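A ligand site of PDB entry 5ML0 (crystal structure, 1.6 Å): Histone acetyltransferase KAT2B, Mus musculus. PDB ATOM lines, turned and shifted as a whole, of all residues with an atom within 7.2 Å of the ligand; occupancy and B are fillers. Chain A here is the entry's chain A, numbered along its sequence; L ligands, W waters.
The backbone NH (N) of Lys 31 lies within hydrogen-bond range of the side-chain carboxylate (OE2) of Glu 34 (2.7 Å).
The side-chain amide nitrogen (ND2) of Asn 81 is in hydrogen-bond range of the backbone carbonyl oxygen (O) of Cys 77, at 2.9 Å.
The backbone carbonyl oxygen of Tyr 87 sits at hydrogen-bond distance from the side-chain sulfur of Cys 77 (3.3 Å).
Water W1 lies within hydrogen-bond range of the side-chain hydroxyl (OH) of Tyr 38 (2.6 Å), an oxygen (O1) of the ligand (2.8 Å) and the backbone NH (N) of Cys 77 (3.3 Å).
Water W2 lies within hydrogen-bond range of the backbone carbonyl oxygen of Glu 34 (2.8 Å) and a nitrogen (N3) of the ligand (3.2 Å).
Water W4 lies within hydrogen-bond range of OH of Tyr 87 and OE1 of Glu 34.
Phe 26 touches the ligand (CE1 to CL1, 3.5 Å).
Pro 29 touches the ligand (O to C4, 3.5 Å).
Val 30 touches the ligand.
Ala 35 touches the ligand.
Tyr 38 touches the ligand.
Cys 77 touches the ligand.
Tyr 80 touches the ligand.
Tyr 87 touches the ligand (CE2 to C8, 3.4 Å).
Hydrophobic or aromatic side chains within 4 Å of the ligand: Pro 25, Phe 26, Val 30, Ala 35, Tyr 38, Tyr 80 and Tyr 87.
Of the 22 residues printed, 11 come within 4 Å of the ligand.
A nitrogen (N1) of the ligand is in salt-bridge range of the side-chain carboxylate (OE1) of Glu 34, at 3.0 Å.
The side-chain amide nitrogen (ND2) of Asn 81 lies within hydrogen-bond range of an oxygen (O1) of the ligand.
The backbone carbonyl oxygen (O) of Pro 25 lies within hydrogen-bond range of a nitrogen (N2) of the ligand (2.9 Å).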
ATOM      1  N   TRP A  24       7.947 -34.694  16.584  1.00  0.00           N
ATOM      2  CA  TRP A  24       8.945 -33.622  16.546  1.00  0.00           C
ATOM      3  C   TRP A  24       8.704 -32.492  15.543  1.00  0.00           C
ATOM      4  O   TRP A  24       9.011 -31.337  15.839  1.00  0.00           O
ATOM      5  CB  TRP A  24      10.379 -34.195  16.417  1.00  0.00           C
ATOM      6  CG  TRP A  24      10.688 -34.805  15.120  1.00  0.00           C
ATOM      7  CD1 TRP A  24      10.614 -36.119  14.787  1.00  0.00           C
ATOM      8  CD2 TRP A  24      11.144 -34.121  13.946  1.00  0.00           C
ATOM      9  NE1 TRP A  24      10.968 -36.314  13.487  1.00  0.00           N
ATOM     10  CE2 TRP A  24      11.299 -35.101  12.939  1.00  0.00           C
ATOM     11  CE3 TRP A  24      11.402 -32.786  13.643  1.00  0.00           C
ATOM     12  CZ2 TRP A  24      11.735 -34.789  11.657  1.00  0.00           C
ATOM     13  CZ3 TRP A  24      11.838 -32.474  12.360  1.00  0.00           C
ATOM     14  CH2 TRP A  24      11.992 -33.464  11.389  1.00  0.00           C
ATOM     15  N   PRO A  25       8.123 -32.797  14.349  1.00  0.00           N
ATOM     16  CA  PRO A  25       7.863 -31.667  13.453  1.00  0.00           C
ATOM     17  C   PRO A  25       6.809 -30.673  13.942  1.00  0.00           C
ATOM     18  O   PRO A  25       6.733 -29.567  13.409  1.00  0.00           O
ATOM     19  CB  PRO A  25       7.373 -32.342  12.158  1.00  0.00           C
ATOM     20  CG  PRO A  25       7.867 -33.744  12.245  1.00  0.00           C
ATOM     21  CD  PRO A  25       7.781 -34.072  13.705  1.00  0.00           C
ATOM     22  N   PHE A  26       6.006 -31.056  14.938  1.00  0.00           N
ATOM     23  CA  PHE A  26       4.789 -30.326  15.305  1.00  0.00           C
ATOM     24  C   PHE A  26       4.868 -29.660  16.677  1.00  0.00           C
ATOM     25  O   PHE A  26       3.857 -29.159  17.171  1.00  0.00           O
ATOM     26  CB  PHE A  26       3.607 -31.301  15.281  1.00  0.00           C
ATOM     27  CG  PHE A  26       3.589 -32.150  14.039  1.00  0.00           C
ATOM     28  CD1 PHE A  26       3.324 -31.575  12.815  1.00  0.00           C
ATOM     29  CD2 PHE A  26       3.894 -33.509  14.089  1.00  0.00           C
ATOM     30  CE1 PHE A  26       3.333 -32.325  11.657  1.00  0.00           C
ATOM     31  CE2 PHE A  26       3.908 -34.276  12.944  1.00  0.00           C
ATOM     32  CZ  PHE A  26       3.635 -33.672  11.717  1.00  0.00           C
ATOM     33  N   MET A  27       6.057 -29.640  17.266  1.00  0.00           N
ATOM     34  CA  MET A  27       6.205 -29.167  18.634  1.00  0.00           C
ATOM     35  C   MET A  27       6.159 -27.648  18.742  1.00  0.00           C
ATOM     36  O   MET A  27       5.762 -27.135  19.781  1.00  0.00           O
ATOM     37  CB  MET A  27       7.505 -29.690  19.246  1.00  0.00           C
ATOM     38  CG  MET A  27       7.575 -31.202  19.343  1.00  0.00           C
ATOM     39  SD  MET A  27       6.297 -31.874  20.420  1.00  0.00           S
ATOM     40  CE  MET A  27       6.991 -31.506  22.024  1.00  0.00           C
ATOM     41  N   GLU A  28       6.547 -26.951  17.675  1.00  0.00           N
ATOM     42  CA  GLU A  28       6.537 -25.497  17.637  1.00  0.00           C
ATOM     43  C   GLU A  28       5.851 -25.025  16.359  1.00  0.00           C
ATOM     44  O   GLU A  28       5.775 -25.778  15.389  1.00  0.00           O
ATOM     45  CB  GLU A  28       7.966 -24.956  17.674  1.00  0.00           C
ATOM     46  CG  GLU A  28       8.753 -25.381  18.901  1.00  0.00           C
ATOM     47  CD  GLU A  28      10.087 -24.673  18.996  1.00  0.00           C
ATOM     48  OE1 GLU A  28      10.837 -24.704  18.009  1.00  0.00           O
ATOM     49  OE2 GLU A  28      10.373 -24.097  20.068  1.00  0.00           O
ATOM     50  N   PRO A  29       5.335 -23.774  16.355  1.00  0.00           N
ATOM     51  CA  PRO A  29       4.720 -23.294  15.130  1.00  0.00           C
ATOM     52  C   PRO A  29       5.704 -23.198  13.957  1.00  0.00           C
ATOM     53  O   PRO A  29       6.899 -22.913  14.152  1.00  0.00           O
ATOM     54  CB  PRO A  29       4.172 -21.910  15.499  1.00  0.00           C
ATOM     55  CG  PRO A  29       4.662 -21.598  16.852  1.00  0.00           C
ATOM     56  CD  PRO A  29       5.149 -22.863  17.488  1.00  0.00           C
ATOM     57  N   VAL A  30       5.191 -23.445  12.767  1.00  0.00           N
ATOM     58  CA  VAL A  30       5.978 -23.342  11.542  1.00  0.00           C
ATOM     59  C   VAL A  30       6.518 -21.911  11.463  1.00  0.00           C
ATOM     60  O   VAL A  30       5.806 -20.954  11.756  1.00  0.00           O
ATOM     61  CB  VAL A  30       5.116 -23.676  10.285  1.00  0.00           C
ATOM     62  CG1 VAL A  30       5.885 -23.398   9.004  1.00  0.00           C
ATOM     63  CG2 VAL A  30       4.645 -25.137  10.313  1.00  0.00           C
ATOM     64  N   LYS A  31       7.798 -21.780  11.114  1.00  0.00           N
ATOM     65  CA  LYS A  31       8.448 -20.480  10.950  1.00  0.00           C
ATOM     66  C   LYS A  31       8.327 -20.042   9.492  1.00  0.00           C
ATOM     67  O   LYS A  31       8.496 -20.851   8.583  1.00  0.00           O
ATOM     68  CB  LYS A  31       9.931 -20.576  11.339  1.00  0.00           C
ATOM     69  CG  LYS A  31      10.148 -20.804  12.822  1.00  0.00           C
ATOM     70  CD  LYS A  31      11.578 -21.202  13.154  1.00  0.00           C
ATOM     71  CE  LYS A  31      12.605 -20.238  12.586  1.00  0.00           C
ATOM     72  NZ  LYS A  31      13.998 -20.621  12.965  1.00  0.00           N
ATOM     73  N   GLU A  34      11.365 -20.869   7.443  1.00  0.00           N
ATOM     74  CA  GLU A  34      11.569 -22.261   7.039  1.00  0.00           C
ATOM     75  C   GLU A  34      10.583 -22.726   5.960  1.00  0.00           C
ATOM     76  O   GLU A  34      10.850 -23.707   5.270  1.00  0.00           O
ATOM     77  CB  GLU A  34      11.561 -23.198   8.260  1.00  0.00           C
ATOM     78  CG  GLU A  34      10.186 -23.662   8.720  1.00  0.00           C
ATOM     79  CD  GLU A  34      10.236 -24.316  10.090  1.00  0.00           C
ATOM     80  OE1 GLU A  34      11.104 -25.195  10.322  1.00  0.00           O
ATOM     81  OE2 GLU A  34       9.413 -23.942  10.934  1.00  0.00           O
ATOM     82  N   ALA A  35       9.455 -22.031   5.800  1.00  0.00           N
ATOM     83  CA  ALA A  35       8.470 -22.404   4.791  1.00  0.00           C
ATOM     84  C   ALA A  35       7.856 -21.156   4.148  1.00  0.00           C
ATOM     85  O   ALA A  35       6.711 -20.801   4.424  1.00  0.00           O
ATOM     86  CB  ALA A  35       7.377 -23.270   5.410  1.00  0.00           C
ATOM     87  N   TYR A  38       3.930 -20.239   3.684  1.00  0.00           N
ATOM     88  CA  TYR A  38       3.089 -21.135   4.495  1.00  0.00           C
ATOM     89  C   TYR A  38       1.881 -20.426   5.072  1.00  0.00           C
ATOM     90  O   TYR A  38       0.772 -20.963   5.042  1.00  0.00           O
ATOM     91  CB  TYR A  38       3.910 -21.740   5.655  1.00  0.00           C
ATOM     92  CG  TYR A  38       3.168 -22.811   6.429  1.00  0.00           C
ATOM     93  CD1 TYR A  38       3.185 -24.133   6.017  1.00  0.00           C
ATOM     94  CD2 TYR A  38       2.453 -22.491   7.585  1.00  0.00           C
ATOM     95  CE1 TYR A  38       2.508 -25.121   6.717  1.00  0.00           C
ATOM     96  CE2 TYR A  38       1.778 -23.473   8.302  1.00  0.00           C
ATOM     97  CZ  TYR A  38       1.805 -24.781   7.865  1.00  0.00           C
ATOM     98  OH  TYR A  38       1.135 -25.757   8.555  1.00  0.00           O
ATOM     99  N   ILE A  42      -1.724 -21.897   4.078  1.00  0.00           N
ATOM    100  CA  ILE A  42      -2.353 -22.567   5.213  1.00  0.00           C
ATOM    101  C   ILE A  42      -3.078 -21.517   6.060  1.00  0.00           C
ATOM    102  O   ILE A  42      -2.447 -20.709   6.762  1.00  0.00           O
ATOM    103  CB  ILE A  42      -1.329 -23.382   6.055  1.00  0.00           C
ATOM    104  CG1 ILE A  42      -0.845 -24.611   5.271  1.00  0.00           C
ATOM    105  CG2 ILE A  42      -1.914 -23.821   7.385  1.00  0.00           C
ATOM    106  CD1 ILE A  42      -1.859 -25.734   5.125  1.00  0.00           C
ATOM    107  N   MET A  46      -1.647 -24.725  13.153  1.00  0.00           N
ATOM    108  CA  MET A  46      -1.737 -25.236  14.502  1.00  0.00           C
ATOM    109  C   MET A  46      -0.499 -26.062  14.805  1.00  0.00           C
ATOM    110  O   MET A  46       0.125 -26.620  13.898  1.00  0.00           O
ATOM    111  CB  MET A  46      -3.008 -26.062  14.697  1.00  0.00           C
ATOM    112  CG  MET A  46      -3.296 -26.479  16.128  1.00  0.00           C
ATOM    113  SD  MET A  46      -3.205 -25.159  17.370  1.00  0.00           S
ATOM    114  CE  MET A  46      -4.356 -23.971  16.681  1.00  0.00           C
ATOM    115  N   VAL A  73      -3.452 -30.015  12.908  1.00  0.00           N
ATOM    116  CA  VAL A  73      -1.983 -30.108  12.891  1.00  0.00           C
ATOM    117  C   VAL A  73      -1.568 -31.025  11.751  1.00  0.00           C
ATOM    118  O   VAL A  73      -0.719 -30.691  10.923  1.00  0.00           O
ATOM    119  CB  VAL A  73      -1.394 -30.652  14.215  1.00  0.00           C
ATOM    120  CG1 VAL A  73       0.107 -30.875  14.082  1.00  0.00           C
ATOM    121  CG2 VAL A  73      -1.657 -29.699  15.371  1.00  0.00           C
ATOM    122  N   ASN A  76      -3.055 -29.940   7.995  1.00  0.00           N
ATOM    123  CA  ASN A  76      -2.224 -28.856   7.456  1.00  0.00           C
ATOM    124  C   ASN A  76      -0.956 -29.423   6.846  1.00  0.00           C
ATOM    125  O   ASN A  76      -0.587 -29.102   5.720  1.00  0.00           O
ATOM    126  CB  ASN A  76      -1.847 -27.834   8.541  1.00  0.00           C
ATOM    127  CG  ASN A  76      -2.978 -26.891   8.901  1.00  0.00           C
ATOM    128  OD1 ASN A  76      -3.999 -26.789   8.209  1.00  0.00           O
ATOM    129  ND2 ASN A  76      -2.803 -26.180  10.008  1.00  0.00           N
ATOM    130  N   CYS A  77      -0.296 -30.279   7.606  1.00  0.00           N
ATOM    131  CA  CYS A  77       0.978 -30.860   7.186  1.00  0.00           C
ATOM    132  C   CYS A  77       0.821 -31.677   5.907  1.00  0.00           C
ATOM    133  O   CYS A  77       1.644 -31.567   4.985  1.00  0.00           O
ATOM    134  CB  CYS A  77       1.545 -31.721   8.302  1.00  0.00           C
ATOM    135  SG  CYS A  77       3.194 -32.348   7.970  1.00  0.00           S
ATOM    136  N   LYS A  78      -0.254 -32.464   5.848  1.00  0.00           N
ATOM    137  CA  LYS A  78      -0.476 -33.377   4.728  1.00  0.00           C
ATOM    138  C   LYS A  78      -1.048 -32.660   3.486  1.00  0.00           C
ATOM    139  O   LYS A  78      -1.001 -33.195   2.394  1.00  0.00           O
ATOM    140  CB  LYS A  78      -1.360 -34.541   5.159  1.00  0.00           C
ATOM    141  CG  LYS A  78      -0.644 -35.483   6.113  1.00  0.00           C
ATOM    142  CD  LYS A  78      -1.537 -36.609   6.587  1.00  0.00           C
ATOM    143  CE  LYS A  78      -1.890 -37.561   5.462  1.00  0.00           C
ATOM    144  NZ  LYS A  78      -2.541 -38.801   5.962  1.00  0.00           N
ATOM    145  N   TYR A  80       0.066 -29.324   2.843  1.00  0.00           N
ATOM    146  CA  TYR A  80       1.191 -28.485   2.416  1.00  0.00           C
ATOM    147  C   TYR A  80       2.357 -29.267   1.808  1.00  0.00           C
ATOM    148  O   TYR A  80       2.915 -28.852   0.791  1.00  0.00           O
ATOM    149  CB  TYR A  80       1.707 -27.658   3.584  1.00  0.00           C
ATOM    150  CG  TYR A  80       2.734 -26.645   3.195  1.00  0.00           C
ATOM    151  CD1 TYR A  80       4.096 -26.963   3.177  1.00  0.00           C
ATOM    152  CD2 TYR A  80       2.358 -25.363   2.821  1.00  0.00           C
ATOM    153  CE1 TYR A  80       5.039 -26.030   2.806  1.00  0.00           C
ATOM    154  CE2 TYR A  80       3.308 -24.418   2.439  1.00  0.00           C
ATOM    155  CZ  TYR A  80       4.640 -24.761   2.439  1.00  0.00           C
ATOM    156  OH  TYR A  80       5.588 -23.820   2.070  1.00  0.00           O
ATOM    157  N   ASN A  81       2.747 -30.361   2.451  1.00  0.00           N
ATOM    158  CA  ASN A  81       3.983 -31.064   2.116  1.00  0.00           C
ATOM    159  C   ASN A  81       3.800 -32.191   1.107  1.00  0.00           C
ATOM    160  O   ASN A  81       2.738 -32.798   1.043  1.00  0.00           O
ATOM    161  CB  ASN A  81       4.612 -31.652   3.373  1.00  0.00           C
ATOM    162  CG  ASN A  81       5.060 -30.575   4.351  1.00  0.00           C
ATOM    163  OD1 ASN A  81       6.115 -29.976   4.185  1.00  0.00           O
ATOM    164  ND2 ASN A  81       4.258 -30.352   5.397  1.00  0.00           N
ATOM    165  N   TYR A  87       8.104 -34.807   6.936  1.00  0.00           N
ATOM    166  CA  TYR A  87       7.015 -34.160   7.679  1.00  0.00           C
ATOM    167  C   TYR A  87       5.669 -34.847   7.416  1.00  0.00           C
ATOM    168  O   TYR A  87       4.937 -35.165   8.352  1.00  0.00           O
ATOM    169  CB  TYR A  87       6.898 -32.660   7.350  1.00  0.00           C
ATOM    170  CG  TYR A  87       8.068 -31.778   7.742  1.00  0.00           C
ATOM    171  CD1 TYR A  87       8.945 -32.128   8.767  1.00  0.00           C
ATOM    172  CD2 TYR A  87       8.274 -30.565   7.089  1.00  0.00           C
ATOM    173  CE1 TYR A  87      10.006 -31.310   9.125  1.00  0.00           C
ATOM    174  CE2 TYR A  87       9.334 -29.733   7.441  1.00  0.00           C
ATOM    175  CZ  TYR A  87      10.194 -30.119   8.455  1.00  0.00           C
ATOM    176  OH  TYR A  87      11.256 -29.314   8.818  1.00  0.00           O
ATOM    177  N   TYR A  88       5.349 -35.059   6.147  1.00  0.00           N
ATOM    178  CA  TYR A  88       4.109 -35.735   5.753  1.00  0.00           C
ATOM    179  C   TYR A  88       4.025 -37.118   6.397  1.00  0.00           C
ATOM    180  O   TYR A  88       2.999 -37.491   6.953  1.00  0.00           O
ATOM    181  CB  TYR A  88       4.059 -35.842   4.236  1.00  0.00           C
ATOM    182  CG  TYR A  88       2.771 -36.382   3.661  1.00  0.00           C
ATOM    183  CD1 TYR A  88       2.464 -37.744   3.749  1.00  0.00           C
ATOM    184  CD2 TYR A  88       1.889 -35.556   2.974  1.00  0.00           C
ATOM    185  CE1 TYR A  88       1.301 -38.251   3.206  1.00  0.00           C
ATOM    186  CE2 TYR A  88       0.717 -36.067   2.422  1.00  0.00           C
ATOM    187  CZ  TYR A  88       0.442 -37.408   2.543  1.00  0.00           C
ATOM    188  OH  TYR A  88      -0.713 -37.930   1.999  1.00  0.00           O
ATOM    189  N   ALA A  91       3.316 -36.905  10.048  1.00  0.00           N
ATOM    190  CA  ALA A  91       1.918 -36.502  10.223  1.00  0.00           C
ATOM    191  C   ALA A  91       0.976 -37.699  10.092  1.00  0.00           C
ATOM    192  O   ALA A  91       0.058 -37.848  10.877  1.00  0.00           O
ATOM    193  CB  ALA A  91       1.548 -35.418   9.236  1.00  0.00           C
HETATM  194  C1  LIG L   1       9.190 -27.801  11.621  1.00  0.00           C
HETATM  195  C2  LIG L   1       8.881 -26.654  12.549  1.00  0.00           C
HETATM  196  C3  LIG L   1       7.396 -28.033   9.911  1.00  0.00           C
HETATM  197  C4  LIG L   1       9.839 -24.861  13.849  1.00  0.00           C
HETATM  198  N1  LIG L   1      10.125 -26.049  13.018  1.00  0.00           N
HETATM  199  C5  LIG L   1      10.902 -27.033  13.784  1.00  0.00           C
HETATM  200  C6  LIG L   1      11.274 -28.203  12.908  1.00  0.00           C
HETATM  201  C7  LIG L   1      10.032 -28.843  12.322  1.00  0.00           C
HETATM  202  N2  LIG L   1       7.942 -28.349  11.082  1.00  0.00           N
HETATM  203  C8  LIG L   1       7.976 -27.032   9.055  1.00  0.00           C
HETATM  204  N3  LIG L   1       7.509 -26.682   7.907  1.00  0.00           N
HETATM  205  N4  LIG L   1       6.374 -27.288   7.460  1.00  0.00           N
HETATM  206  C9  LIG L   1       5.919 -26.837   6.151  1.00  0.00           C
HETATM  207  C10 LIG L   1       5.677 -28.257   8.130  1.00  0.00           C
HETATM  208  O1  LIG L   1       4.667 -28.751   7.643  1.00  0.00           O
HETATM  209  C11 LIG L   1       6.234 -28.609   9.406  1.00  0.00           C
HETATM  210 CL1  LIG L   1       5.392 -29.819  10.308  1.00  0.00          CL
HETATM  211  O   HOH W   1       2.109 -28.142   8.539  1.00  0.00           O
HETATM  212  O   HOH W   2       9.960 -26.299   5.874  1.00  0.00           O
HETATM  213  O   HOH W   3       8.712 -28.530  16.047  1.00  0.00           O
HETATM  214  O   HOH W   4      12.803 -27.924  10.058  1.00  0.00           O
